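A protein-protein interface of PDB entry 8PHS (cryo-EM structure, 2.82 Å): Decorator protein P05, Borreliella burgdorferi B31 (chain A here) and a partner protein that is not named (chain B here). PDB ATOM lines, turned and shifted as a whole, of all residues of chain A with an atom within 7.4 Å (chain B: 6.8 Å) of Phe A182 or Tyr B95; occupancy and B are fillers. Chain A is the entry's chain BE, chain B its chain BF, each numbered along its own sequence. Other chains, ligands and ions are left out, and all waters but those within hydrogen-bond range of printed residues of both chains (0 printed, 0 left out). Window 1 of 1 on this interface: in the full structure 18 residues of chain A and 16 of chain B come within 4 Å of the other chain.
The side-chain amide oxygen of Asn A121 is in hydrogen-bond range of the side-chain hydroxyl of Thr B114 (3.3 Å).
The guanidinium group (NH2) of Arg A52 lies within hydrogen-bond range of the side-chain hydroxyl (OH) of Tyr B62 (3.0 Å).
OE1 of Glu B60 is in salt-bridge range of NH2 of Arg A52 (3.9 Å).
The side-chain carboxylate (OE2) of Glu B60 lies within hydrogen-bond range of the side-chain amide nitrogen (ND2) of Asn A121 (2.9 Å).
OE2 of Glu A123 is in hydrogen-bond range of OH of Tyr B95 (3.3 Å).
OD1 of Asp B93 lies within salt-bridge range of NZ of Lys A138 (3.3 Å).
The side-chain carboxylate (OE2) of Glu A123 lies within hydrogen-bond range of the side-chain hydroxyl (OH) of Tyr B62 (3.0 Å).
O of Asn A160 is in hydrogen-bond range of N of Phe A182 (3.0 Å).
OD1 of Asn A160 sits close to O of Asn A184.
The side-chain amide oxygen (OD1) of Asn A120 lies close to the side-chain amide oxygen (OD1) of Asn A121, at 3.4 Å.
The backbone NH (N) of Lys A185 lies within hydrogen-bond range of the side-chain amide oxygen (OD1) of Asn A160.
The backbone NH (N) of Val B110 is in hydrogen-bond range of the backbone carbonyl oxygen (O) of Glu B60 (2.9 Å).
The backbone NH of Ile B113 sits at hydrogen-bond distance from the backbone carbonyl oxygen of Tyr B95, at 3.1 Å.
Thr B114 touches Thr A119 (CB to O, 3.6 Å).
Asn A160 touches Asp B92.
CE2 of Phe A182 touches O of Leu B94, 3.3 Å away.
Phe A182 touches Tyr B95 (CG to CD1, 3.6 Å).
Phe A182 touches Thr B114 (C to CG2, 3.8 Å).
Thr B114 touches Gly A183 (CG2 to N, 3.3 Å).
Printed residues of chain B within 4 Å of Asn A160: Asp B92.
Of chain B, only Leu B94 (3.3 Å), Tyr B95 (3.6 Å) and Thr B114 (3.8 Å) come within 4 Å of Phe A182.
Of the printed residues of chain B, Gly A183 touches Thr B114 (3.3 Å).
Lys B74 touches none of the printed residues of chain A.
Of the printed residues of chain A, Tyr B95 touches Glu A123 and Phe A182.
Ile B113 touches none of the printed residues of chain A.
The nearest residue of chain B that does not touch Phe A182 is Ile B113 (4.2 Å).
The nearest printed residue of chain B that does not touch Asn A121 is Pro B112 (4.03 Å).
Of the 21 printed residues of chain B, 7 touch a printed residue of chain A.
Hydrophobic or aromatic side chains of chain B within 4 Å of the printed part of chain A: Tyr B62 and Tyr B95.
Of the 19 printed residues of chain A, 8 touch a printed residue of chain B.
Printed residues of chain A that touch a printed residue of chain B: Arg A52, Thr A119, Asn A121, Glu A123, Lys A138, Asn A160, Phe A182 and Gly A183.
Hydrophobic or aromatic side chains of chain A that line the printed part of chain B: Phe A182.
Among the printed residues, 13 pairs touch across the chains.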
ATOM      1  N   ARG A  52      21.083   9.545  14.135  1.00  0.00           N
ATOM      2  CA  ARG A  52      20.140  10.220  15.017  1.00  0.00           C
ATOM      3  C   ARG A  52      19.058  10.865  14.166  1.00  0.00           C
ATOM      4  O   ARG A  52      19.361  11.641  13.255  1.00  0.00           O
ATOM      5  CB  ARG A  52      20.838  11.273  15.879  1.00  0.00           C
ATOM      6  CG  ARG A  52      21.855  10.702  16.851  1.00  0.00           C
ATOM      7  CD  ARG A  52      22.900  11.739  17.213  1.00  0.00           C
ATOM      8  NE  ARG A  52      22.293  13.001  17.616  1.00  0.00           N
ATOM      9  CZ  ARG A  52      22.970  14.119  17.838  1.00  0.00           C
ATOM     10  NH1 ARG A  52      24.283  14.174  17.689  1.00  0.00           N
ATOM     11  NH2 ARG A  52      22.312  15.212  18.215  1.00  0.00           N
ATOM     12  N   ILE A 118      18.138  20.014   1.798  1.00  0.00           N
ATOM     13  CA  ILE A 118      19.295  20.696   2.360  1.00  0.00           C
ATOM     14  C   ILE A 118      18.908  21.734   3.405  1.00  0.00           C
ATOM     15  O   ILE A 118      19.772  22.211   4.145  1.00  0.00           O
ATOM     16  CB  ILE A 118      20.127  21.341   1.230  1.00  0.00           C
ATOM     17  CG1 ILE A 118      21.561  21.598   1.696  1.00  0.00           C
ATOM     18  CG2 ILE A 118      19.477  22.630   0.757  1.00  0.00           C
ATOM     19  CD1 ILE A 118      22.279  20.353   2.164  1.00  0.00           C
ATOM     20  N   THR A 119      17.628  22.090   3.491  1.00  0.00           N
ATOM     21  CA  THR A 119      17.153  22.983   4.538  1.00  0.00           C
ATOM     22  C   THR A 119      16.937  22.267   5.864  1.00  0.00           C
ATOM     23  O   THR A 119      16.554  22.914   6.844  1.00  0.00           O
ATOM     24  CB  THR A 119      15.850  23.658   4.105  1.00  0.00           C
ATOM     25  OG1 THR A 119      14.837  22.665   3.902  1.00  0.00           O
ATOM     26  CG2 THR A 119      16.058  24.431   2.816  1.00  0.00           C
ATOM     27  N   ASN A 120      17.171  20.958   5.914  1.00  0.00           N
ATOM     28  CA  ASN A 120      17.030  20.163   7.125  1.00  0.00           C
ATOM     29  C   ASN A 120      18.361  19.492   7.425  1.00  0.00           C
ATOM     30  O   ASN A 120      18.972  18.894   6.533  1.00  0.00           O
ATOM     31  CB  ASN A 120      15.924  19.119   6.961  1.00  0.00           C
ATOM     32  CG  ASN A 120      15.491  18.517   8.279  1.00  0.00           C
ATOM     33  OD1 ASN A 120      16.012  18.870   9.336  1.00  0.00           O
ATOM     34  ND2 ASN A 120      14.528  17.607   8.225  1.00  0.00           N
ATOM     35  N   ASN A 121      18.810  19.595   8.673  1.00  0.00           N
ATOM     36  CA  ASN A 121      20.100  19.030   9.044  1.00  0.00           C
ATOM     37  C   ASN A 121      20.027  17.507   9.100  1.00  0.00           C
ATOM     38  O   ASN A 121      18.961  16.917   9.297  1.00  0.00           O
ATOM     39  CB  ASN A 121      20.565  19.591  10.387  1.00  0.00           C
ATOM     40  CG  ASN A 121      19.650  19.210  11.525  1.00  0.00           C
ATOM     41  OD1 ASN A 121      18.477  19.576  11.543  1.00  0.00           O
ATOM     42  ND2 ASN A 121      20.187  18.481  12.496  1.00  0.00           N
ATOM     43  N   PHE A 122      21.182  16.870   8.918  1.00  0.00           N
ATOM     44  CA  PHE A 122      21.257  15.422   8.804  1.00  0.00           C
ATOM     45  C   PHE A 122      22.512  14.912   9.498  1.00  0.00           C
ATOM     46  O   PHE A 122      23.539  15.594   9.540  1.00  0.00           O
ATOM     47  CB  PHE A 122      21.259  14.989   7.331  1.00  0.00           C
ATOM     48  CG  PHE A 122      21.464  13.516   7.129  1.00  0.00           C
ATOM     49  CD1 PHE A 122      20.458  12.616   7.431  1.00  0.00           C
ATOM     50  CD2 PHE A 122      22.667  13.033   6.644  1.00  0.00           C
ATOM     51  CE1 PHE A 122      20.645  11.262   7.245  1.00  0.00           C
ATOM     52  CE2 PHE A 122      22.861  11.681   6.458  1.00  0.00           C
ATOM     53  CZ  PHE A 122      21.848  10.793   6.759  1.00  0.00           C
ATOM     54  N   GLU A 123      22.414  13.700  10.044  1.00  0.00           N
ATOM     55  CA  GLU A 123      23.547  13.011  10.655  1.00  0.00           C
ATOM     56  C   GLU A 123      23.497  11.549  10.242  1.00  0.00           C
ATOM     57  O   GLU A 123      22.496  10.870  10.491  1.00  0.00           O
ATOM     58  CB  GLU A 123      23.525  13.136  12.183  1.00  0.00           C
ATOM     59  CG  GLU A 123      23.483  14.565  12.702  1.00  0.00           C
ATOM     60  CD  GLU A 123      23.967  14.680  14.134  1.00  0.00           C
ATOM     61  OE1 GLU A 123      24.433  13.662  14.688  1.00  0.00           O
ATOM     62  OE2 GLU A 123      23.879  15.787  14.706  1.00  0.00           O
ATOM     63  N   LYS A 138      36.238  19.447   7.039  1.00  0.00           N
ATOM     64  CA  LYS A 138      35.081  20.017   6.361  1.00  0.00           C
ATOM     65  C   LYS A 138      35.008  19.454   4.949  1.00  0.00           C
ATOM     66  O   LYS A 138      36.036  19.275   4.289  1.00  0.00           O
ATOM     67  CB  LYS A 138      35.160  21.543   6.330  1.00  0.00           C
ATOM     68  CG  LYS A 138      34.946  22.188   7.687  1.00  0.00           C
ATOM     69  CD  LYS A 138      35.057  23.700   7.615  1.00  0.00           C
ATOM     70  CE  LYS A 138      34.844  24.328   8.984  1.00  0.00           C
ATOM     71  NZ  LYS A 138      35.144  25.784   8.977  1.00  0.00           N
ATOM     72  N   ILE A 159      28.161  24.429   1.447  1.00  0.00           N
ATOM     73  CA  ILE A 159      27.360  23.929   2.554  1.00  0.00           C
ATOM     74  C   ILE A 159      28.292  23.568   3.701  1.00  0.00           C
ATOM     75  O   ILE A 159      29.497  23.377   3.519  1.00  0.00           O
ATOM     76  CB  ILE A 159      26.501  22.709   2.162  1.00  0.00           C
ATOM     77  CG1 ILE A 159      27.397  21.522   1.805  1.00  0.00           C
ATOM     78  CG2 ILE A 159      25.571  23.049   1.009  1.00  0.00           C
ATOM     79  CD1 ILE A 159      26.696  20.190   1.883  1.00  0.00           C
ATOM     80  N   ASN A 160      27.716  23.474   4.897  1.00  0.00           N
ATOM     81  CA  ASN A 160      28.454  23.055   6.083  1.00  0.00           C
ATOM     82  C   ASN A 160      28.286  21.551   6.260  1.00  0.00           C
ATOM     83  O   ASN A 160      27.192  21.073   6.575  1.00  0.00           O
ATOM     84  CB  ASN A 160      27.977  23.804   7.324  1.00  0.00           C
ATOM     85  CG  ASN A 160      28.072  25.304   7.174  1.00  0.00           C
ATOM     86  OD1 ASN A 160      27.296  25.916   6.444  1.00  0.00           O
ATOM     87  ND2 ASN A 160      29.026  25.908   7.871  1.00  0.00           N
ATOM     88  N   ALA A 161      29.370  20.810   6.052  1.00  0.00           N
ATOM     89  CA  ALA A 161      29.404  19.379   6.313  1.00  0.00           C
ATOM     90  C   ALA A 161      30.695  19.065   7.049  1.00  0.00           C
ATOM     91  O   ALA A 161      31.782  19.390   6.565  1.00  0.00           O
ATOM     92  CB  ALA A 161      29.316  18.565   5.017  1.00  0.00           C
ATOM     93  N   THR A 162      30.571  18.441   8.217  1.00  0.00           N
ATOM     94  CA  THR A 162      31.711  18.119   9.063  1.00  0.00           C
ATOM     95  C   THR A 162      31.791  16.612   9.244  1.00  0.00           C
ATOM     96  O   THR A 162      30.793  15.971   9.589  1.00  0.00           O
ATOM     97  CB  THR A 162      31.601  18.808  10.426  1.00  0.00           C
ATOM     98  OG1 THR A 162      31.397  20.215  10.239  1.00  0.00           O
ATOM     99  CG2 THR A 162      32.868  18.591  11.234  1.00  0.00           C
ATOM    100  N   VAL A 179      28.975  11.877   8.877  1.00  0.00           N
ATOM    101  CA  VAL A 179      29.015  13.302   8.572  1.00  0.00           C
ATOM    102  C   VAL A 179      27.765  13.968   9.126  1.00  0.00           C
ATOM    103  O   VAL A 179      26.660  13.426   9.022  1.00  0.00           O
ATOM    104  CB  VAL A 179      29.137  13.546   7.053  1.00  0.00           C
ATOM    105  CG1 VAL A 179      28.919  15.013   6.714  1.00  0.00           C
ATOM    106  CG2 VAL A 179      30.490  13.089   6.554  1.00  0.00           C
ATOM    107  N   ALA A 180      27.943  15.147   9.715  1.00  0.00           N
ATOM    108  CA  ALA A 180      26.837  16.001  10.121  1.00  0.00           C
ATOM    109  C   ALA A 180      26.723  17.148   9.125  1.00  0.00           C
ATOM    110  O   ALA A 180      27.641  17.966   9.006  1.00  0.00           O
ATOM    111  CB  ALA A 180      27.045  16.535  11.538  1.00  0.00           C
ATOM    112  N   VAL A 181      25.602  17.204   8.413  1.00  0.00           N
ATOM    113  CA  VAL A 181      25.342  18.243   7.424  1.00  0.00           C
ATOM    114  C   VAL A 181      24.317  19.194   8.019  1.00  0.00           C
ATOM    115  O   VAL A 181      23.189  18.792   8.326  1.00  0.00           O
ATOM    116  CB  VAL A 181      24.846  17.652   6.096  1.00  0.00           C
ATOM    117  CG1 VAL A 181      24.655  18.753   5.068  1.00  0.00           C
ATOM    118  CG2 VAL A 181      25.827  16.616   5.585  1.00  0.00           C
ATOM    119  N   PHE A 182      24.707  20.456   8.186  1.00  0.00           N
ATOM    120  CA  PHE A 182      23.866  21.459   8.836  1.00  0.00           C
ATOM    121  C   PHE A 182      23.884  22.728   7.983  1.00  0.00           C
ATOM    122  O   PHE A 182      24.771  23.575   8.102  1.00  0.00           O
ATOM    123  CB  PHE A 182      24.324  21.695  10.286  1.00  0.00           C
ATOM    124  CG  PHE A 182      25.756  22.135  10.422  1.00  0.00           C
ATOM    125  CD1 PHE A 182      26.783  21.210  10.391  1.00  0.00           C
ATOM    126  CD2 PHE A 182      26.069  23.462  10.663  1.00  0.00           C
ATOM    127  CE1 PHE A 182      28.094  21.607  10.529  1.00  0.00           C
ATOM    128  CE2 PHE A 182      27.377  23.863  10.805  1.00  0.00           C
ATOM    129  CZ  PHE A 182      28.391  22.933  10.741  1.00  0.00           C
ATOM    130  N   GLY A 183      22.912  22.839   7.085  1.00  0.00           N
ATOM    131  CA  GLY A 183      22.717  24.072   6.353  1.00  0.00           C
ATOM    132  C   GLY A 183      23.777  24.344   5.295  1.00  0.00           C
ATOM    133  O   GLY A 183      24.513  23.466   4.850  1.00  0.00           O
ATOM    134  N   ASN A 184      23.831  25.613   4.896  1.00  0.00           N
ATOM    135  CA  ASN A 184      24.708  26.081   3.837  1.00  0.00           C
ATOM    136  C   ASN A 184      25.608  27.203   4.338  1.00  0.00           C
ATOM    137  O   ASN A 184      25.302  27.873   5.331  1.00  0.00           O
ATOM    138  CB  ASN A 184      23.890  26.537   2.617  1.00  0.00           C
ATOM    139  CG  ASN A 184      22.983  27.729   2.907  1.00  0.00           C
ATOM    140  OD1 ASN A 184      23.020  28.332   3.977  1.00  0.00           O
ATOM    141  ND2 ASN A 184      22.139  28.052   1.947  1.00  0.00           N
ATOM    142  N   LYS A 185      26.737  27.382   3.663  1.00  0.00           N
ATOM    143  CA  LYS A 185      27.643  28.462   4.005  1.00  0.00           C
ATOM    144  C   LYS A 185      27.183  29.770   3.369  1.00  0.00           C
ATOM    145  O   LYS A 185      26.455  29.787   2.372  1.00  0.00           O
ATOM    146  CB  LYS A 185      29.068  28.131   3.562  1.00  0.00           C
ATOM    147  CG  LYS A 185      29.655  26.911   4.246  1.00  0.00           C
ATOM    148  CD  LYS A 185      31.122  26.729   3.886  1.00  0.00           C
ATOM    149  CE  LYS A 185      31.755  25.629   4.721  1.00  0.00           C
ATOM    150  NZ  LYS A 185      33.202  25.447   4.416  1.00  0.00           N
ATOM    151  N   GLU B  60      17.761  19.152  19.777  1.00  0.00           N
ATOM    152  CA  GLU B  60      18.787  18.165  20.068  1.00  0.00           C
ATOM    153  C   GLU B  60      19.382  18.449  21.440  1.00  0.00           C
ATOM    154  O   GLU B  60      19.168  19.511  22.023  1.00  0.00           O
ATOM    155  CB  GLU B  60      19.881  18.186  18.993  1.00  0.00           C
ATOM    156  CG  GLU B  60      19.363  17.958  17.584  1.00  0.00           C
ATOM    157  CD  GLU B  60      20.396  18.281  16.524  1.00  0.00           C
ATOM    158  OE1 GLU B  60      21.480  18.786  16.883  1.00  0.00           O
ATOM    159  OE2 GLU B  60      20.127  18.030  15.332  1.00  0.00           O
ATOM    160  N   TYR B  62      23.250  17.873  23.650  1.00  0.00           N
ATOM    161  CA  TYR B  62      24.665  17.568  23.509  1.00  0.00           C
ATOM    162  C   TYR B  62      25.350  17.691  24.860  1.00  0.00           C
ATOM    163  O   TYR B  62      24.844  18.367  25.761  1.00  0.00           O
ATOM    164  CB  TYR B  62      25.340  18.511  22.504  1.00  0.00           C
ATOM    165  CG  TYR B  62      24.951  18.264  21.067  1.00  0.00           C
ATOM    166  CD1 TYR B  62      25.538  17.243  20.332  1.00  0.00           C
ATOM    167  CD2 TYR B  62      23.990  19.048  20.445  1.00  0.00           C
ATOM    168  CE1 TYR B  62      25.183  17.016  19.019  1.00  0.00           C
ATOM    169  CE2 TYR B  62      23.629  18.827  19.134  1.00  0.00           C
ATOM    170  CZ  TYR B  62      24.228  17.810  18.425  1.00  0.00           C
ATOM    171  OH  TYR B  62      23.869  17.587  17.116  1.00  0.00           O
ATOM    172  N   GLY B  72      25.430  31.166  21.025  1.00  0.00           N
ATOM    173  CA  GLY B  72      25.655  30.329  19.861  1.00  0.00           C
ATOM    174  C   GLY B  72      26.709  29.276  20.156  1.00  0.00           C
ATOM    175  O   GLY B  72      27.709  29.536  20.824  1.00  0.00           O
ATOM    176  N   VAL B  73      26.485  28.073  19.638  1.00  0.00           N
ATOM    177  CA  VAL B  73      27.345  26.940  19.950  1.00  0.00           C
ATOM    178  C   VAL B  73      27.963  26.398  18.672  1.00  0.00           C
ATOM    179  O   VAL B  73      27.429  26.562  17.571  1.00  0.00           O
ATOM    180  CB  VAL B  73      26.581  25.823  20.694  1.00  0.00           C
ATOM    181  CG1 VAL B  73      26.086  26.327  22.033  1.00  0.00           C
ATOM    182  CG2 VAL B  73      25.427  25.313  19.848  1.00  0.00           C
ATOM    183  N   LYS B  74      29.112  25.749  18.836  1.00  0.00           N
ATOM    184  CA  LYS B  74      29.809  25.065  17.762  1.00  0.00           C
ATOM    185  C   LYS B  74      30.247  23.695  18.258  1.00  0.00           C
ATOM    186  O   LYS B  74      30.366  23.453  19.463  1.00  0.00           O
ATOM    187  CB  LYS B  74      31.026  25.858  17.274  1.00  0.00           C
ATOM    188  CG  LYS B  74      32.048  26.146  18.357  1.00  0.00           C
ATOM    189  CD  LYS B  74      33.230  26.918  17.805  1.00  0.00           C
ATOM    190  CE  LYS B  74      34.209  27.284  18.906  1.00  0.00           C
ATOM    191  NZ  LYS B  74      35.406  27.984  18.368  1.00  0.00           N
ATOM    192  N   LEU B  75      30.493  22.800  17.306  1.00  0.00           N
ATOM    193  CA  LEU B  75      30.898  21.437  17.621  1.00  0.00           C
ATOM    194  C   LEU B  75      32.381  21.413  17.965  1.00  0.00           C
ATOM    195  O   LEU B  75      33.215  21.875  17.180  1.00  0.00           O
ATOM    196  CB  LEU B  75      30.604  20.509  16.444  1.00  0.00           C
ATOM    197  CG  LEU B  75      29.135  20.192  16.160  1.00  0.00           C
ATOM    198  CD1 LEU B  75      29.023  19.051  15.164  1.00  0.00           C
ATOM    199  CD2 LEU B  75      28.397  19.857  17.443  1.00  0.00           C
ATOM    200  N   VAL B  86      29.557  20.411  22.570  1.00  0.00           N
ATOM    201  CA  VAL B  86      29.285  21.745  22.050  1.00  0.00           C
ATOM    202  C   VAL B  86      29.910  22.775  22.978  1.00  0.00           C
ATOM    203  O   VAL B  86      29.856  22.638  24.204  1.00  0.00           O
ATOM    204  CB  VAL B  86      27.773  22.005  21.879  1.00  0.00           C
ATOM    205  CG1 VAL B  86      27.208  21.126  20.776  1.00  0.00           C
ATOM    206  CG2 VAL B  86      27.031  21.765  23.182  1.00  0.00           C
ATOM    207  N   GLY B  89      30.594  29.594  20.789  1.00  0.00           N
ATOM    208  CA  GLY B  89      31.371  30.033  19.645  1.00  0.00           C
ATOM    209  C   GLY B  89      30.453  30.517  18.545  1.00  0.00           C
ATOM    210  O   GLY B  89      29.230  30.580  18.704  1.00  0.00           O
ATOM    211  N   GLY B  90      31.066  30.858  17.417  1.00  0.00           N
ATOM    212  CA  GLY B  90      30.314  31.365  16.287  1.00  0.00           C
ATOM    213  C   GLY B  90      31.141  31.522  15.030  1.00  0.00           C
ATOM    214  O   GLY B  90      32.137  30.818  14.841  1.00  0.00           O
ATOM    215  N   GLY B  91      30.738  32.445  14.161  1.00  0.00           N
ATOM    216  CA  GLY B  91      31.440  32.661  12.913  1.00  0.00           C
ATOM    217  C   GLY B  91      31.142  31.592  11.884  1.00  0.00           C
ATOM    218  O   GLY B  91      29.992  31.168  11.735  1.00  0.00           O
ATOM    219  N   ASP B  92      32.173  31.143  11.169  1.00  0.00           N
ATOM    220  CA  ASP B  92      32.003  30.100  10.165  1.00  0.00           C
ATOM    221  C   ASP B  92      31.785  28.722  10.772  1.00  0.00           C
ATOM    222  O   ASP B  92      31.444  27.788  10.038  1.00  0.00           O
ATOM    223  CB  ASP B  92      33.220  30.060   9.238  1.00  0.00           C
ATOM    224  CG  ASP B  92      33.663  31.440   8.799  1.00  0.00           C
ATOM    225  OD1 ASP B  92      32.869  32.136   8.131  1.00  0.00           O
ATOM    226  OD2 ASP B  92      34.804  31.830   9.122  1.00  0.00           O
ATOM    227  N   ASP B  93      31.973  28.571  12.081  1.00  0.00           N
ATOM    228  CA  ASP B  93      31.819  27.291  12.755  1.00  0.00           C
ATOM    229  C   ASP B  93      30.495  27.166  13.494  1.00  0.00           C
ATOM    230  O   ASP B  93      30.272  26.153  14.163  1.00  0.00           O
ATOM    231  CB  ASP B  93      32.974  27.072  13.736  1.00  0.00           C
ATOM    232  CG  ASP B  93      34.329  27.130  13.063  1.00  0.00           C
ATOM    233  OD1 ASP B  93      34.373  27.291  11.825  1.00  0.00           O
ATOM    234  OD2 ASP B  93      35.352  27.018  13.770  1.00  0.00           O
ATOM    235  N   LEU B  94      29.619  28.164  13.394  1.00  0.00           N
ATOM    236  CA  LEU B  94      28.364  28.144  14.133  1.00  0.00           C
ATOM    237  C   LEU B  94      27.526  26.933  13.746  1.00  0.00           C
ATOM    238  O   LEU B  94      27.338  26.642  12.561  1.00  0.00           O
ATOM    239  CB  LEU B  94      27.582  29.431  13.876  1.00  0.00           C
ATOM    240  CG  LEU B  94      26.280  29.577  14.665  1.00  0.00           C
ATOM    241  CD1 LEU B  94      26.564  30.014  16.092  1.00  0.00           C
ATOM    242  CD2 LEU B  94      25.337  30.553  13.981  1.00  0.00           C
ATOM    243  N   TYR B  95      27.020  26.229  14.755  1.00  0.00           N
ATOM    244  CA  TYR B  95      26.199  25.044  14.549  1.00  0.00           C
ATOM    245  C   TYR B  95      24.755  25.219  14.986  1.00  0.00           C
ATOM    246  O   TYR B  95      23.866  24.615  14.386  1.00  0.00           O
ATOM    247  CB  TYR B  95      26.801  23.847  15.298  1.00  0.00           C
ATOM    248  CG  TYR B  95      26.016  22.567  15.138  1.00  0.00           C
ATOM    249  CD1 TYR B  95      26.096  21.824  13.970  1.00  0.00           C
ATOM    250  CD2 TYR B  95      25.190  22.104  16.152  1.00  0.00           C
ATOM    251  CE1 TYR B  95      25.381  20.655  13.816  1.00  0.00           C
ATOM    252  CE2 TYR B  95      24.469  20.937  16.008  1.00  0.00           C
ATOM    253  CZ  TYR B  95      24.570  20.216  14.837  1.00  0.00           C
ATOM    254  OH  TYR B  95      23.855  19.051  14.686  1.00  0.00           O
ATOM    255  N   GLY B  96      24.502  26.028  16.006  1.00  0.00           N
ATOM    256  CA  GLY B  96      23.147  26.213  16.481  1.00  0.00           C
ATOM    257  C   GLY B  96      23.120  27.159  17.661  1.00  0.00           C
ATOM    258  O   GLY B  96      24.106  27.834  17.964  1.00  0.00           O
ATOM    259  N   VAL B  97      21.969  27.198  18.326  1.00  0.00           N
ATOM    260  CA  VAL B  97      21.747  28.069  19.473  1.00  0.00           C
ATOM    261  C   VAL B  97      21.387  27.209  20.676  1.00  0.00           C
ATOM    262  O   VAL B  97      20.487  26.366  20.595  1.00  0.00           O
ATOM    263  CB  VAL B  97      20.639  29.102  19.195  1.00  0.00           C
ATOM    264  CG1 VAL B  97      20.316  29.885  20.455  1.00  0.00           C
ATOM    265  CG2 VAL B  97      21.058  30.039  18.075  1.00  0.00           C
ATOM    266  N   VAL B 110      20.044  22.218  22.218  1.00  0.00           N
ATOM    267  CA  VAL B 110      20.487  22.980  21.060  1.00  0.00           C
ATOM    268  C   VAL B 110      19.397  22.954  19.997  1.00  0.00           C
ATOM    269  O   VAL B 110      18.786  21.910  19.735  1.00  0.00           O
ATOM    270  CB  VAL B 110      21.813  22.427  20.499  1.00  0.00           C
ATOM    271  CG1 VAL B 110      22.256  23.220  19.282  1.00  0.00           C
ATOM    272  CG2 VAL B 110      22.889  22.443  21.571  1.00  0.00           C
ATOM    273  N   ILE B 111      19.144  24.112  19.405  1.00  0.00           N
ATOM    274  CA  ILE B 111      18.309  24.259  18.220  1.00  0.00           C
ATOM    275  C   ILE B 111      19.242  24.478  17.033  1.00  0.00           C
ATOM    276  O   ILE B 111      20.024  25.438  17.041  1.00  0.00           O
ATOM    277  CB  ILE B 111      17.313  25.419  18.365  1.00  0.00           C
ATOM    278  CG1 ILE B 111      16.306  25.108  19.474  1.00  0.00           C
ATOM    279  CG2 ILE B 111      16.599  25.674  17.050  1.00  0.00           C
ATOM    280  CD1 ILE B 111      15.213  26.137  19.615  1.00  0.00           C
ATOM    281  N   PRO B 112      19.215  23.614  16.020  1.00  0.00           N
ATOM    282  CA  PRO B 112      20.178  23.729  14.919  1.00  0.00           C
ATOM    283  C   PRO B 112      19.979  25.009  14.123  1.00  0.00           C
ATOM    284  O   PRO B 112      18.905  25.613  14.114  1.00  0.00           O
ATOM    285  CB  PRO B 112      19.885  22.492  14.062  1.00  0.00           C
ATOM    286  CG  PRO B 112      19.187  21.545  14.983  1.00  0.00           C
ATOM    287  CD  PRO B 112      18.376  22.413  15.891  1.00  0.00           C
ATOM    288  N   ILE B 113      21.053  25.425  13.447  1.00  0.00           N
ATOM    289  CA  ILE B 113      21.011  26.632  12.630  1.00  0.00           C
ATOM    290  C   ILE B 113      20.081  26.496  11.436  1.00  0.00           C
ATOM    291  O   ILE B 113      19.723  27.506  10.821  1.00  0.00           O
ATOM    292  CB  ILE B 113      22.434  27.005  12.163  1.00  0.00           C
ATOM    293  CG1 ILE B 113      22.509  28.488  11.803  1.00  0.00           C
ATOM    294  CG2 ILE B 113      22.856  26.144  10.986  1.00  0.00           C
ATOM    295  CD1 ILE B 113      22.012  29.403  12.897  1.00  0.00           C
ATOM    296  N   THR B 114      19.666  25.276  11.100  1.00  0.00           N
ATOM    297  CA  THR B 114      18.697  25.056  10.036  1.00  0.00           C
ATOM    298  C   THR B 114      17.263  25.263  10.498  1.00  0.00           C
ATOM    299  O   THR B 114      16.345  25.173   9.676  1.00  0.00           O
ATOM    300  CB  THR B 114      18.847  23.642   9.471  1.00  0.00           C
ATOM    301  OG1 THR B 114      18.607  22.685  10.508  1.00  0.00           O
ATOM    302  CG2 THR B 114      20.244  23.440   8.924  1.00  0.00           C
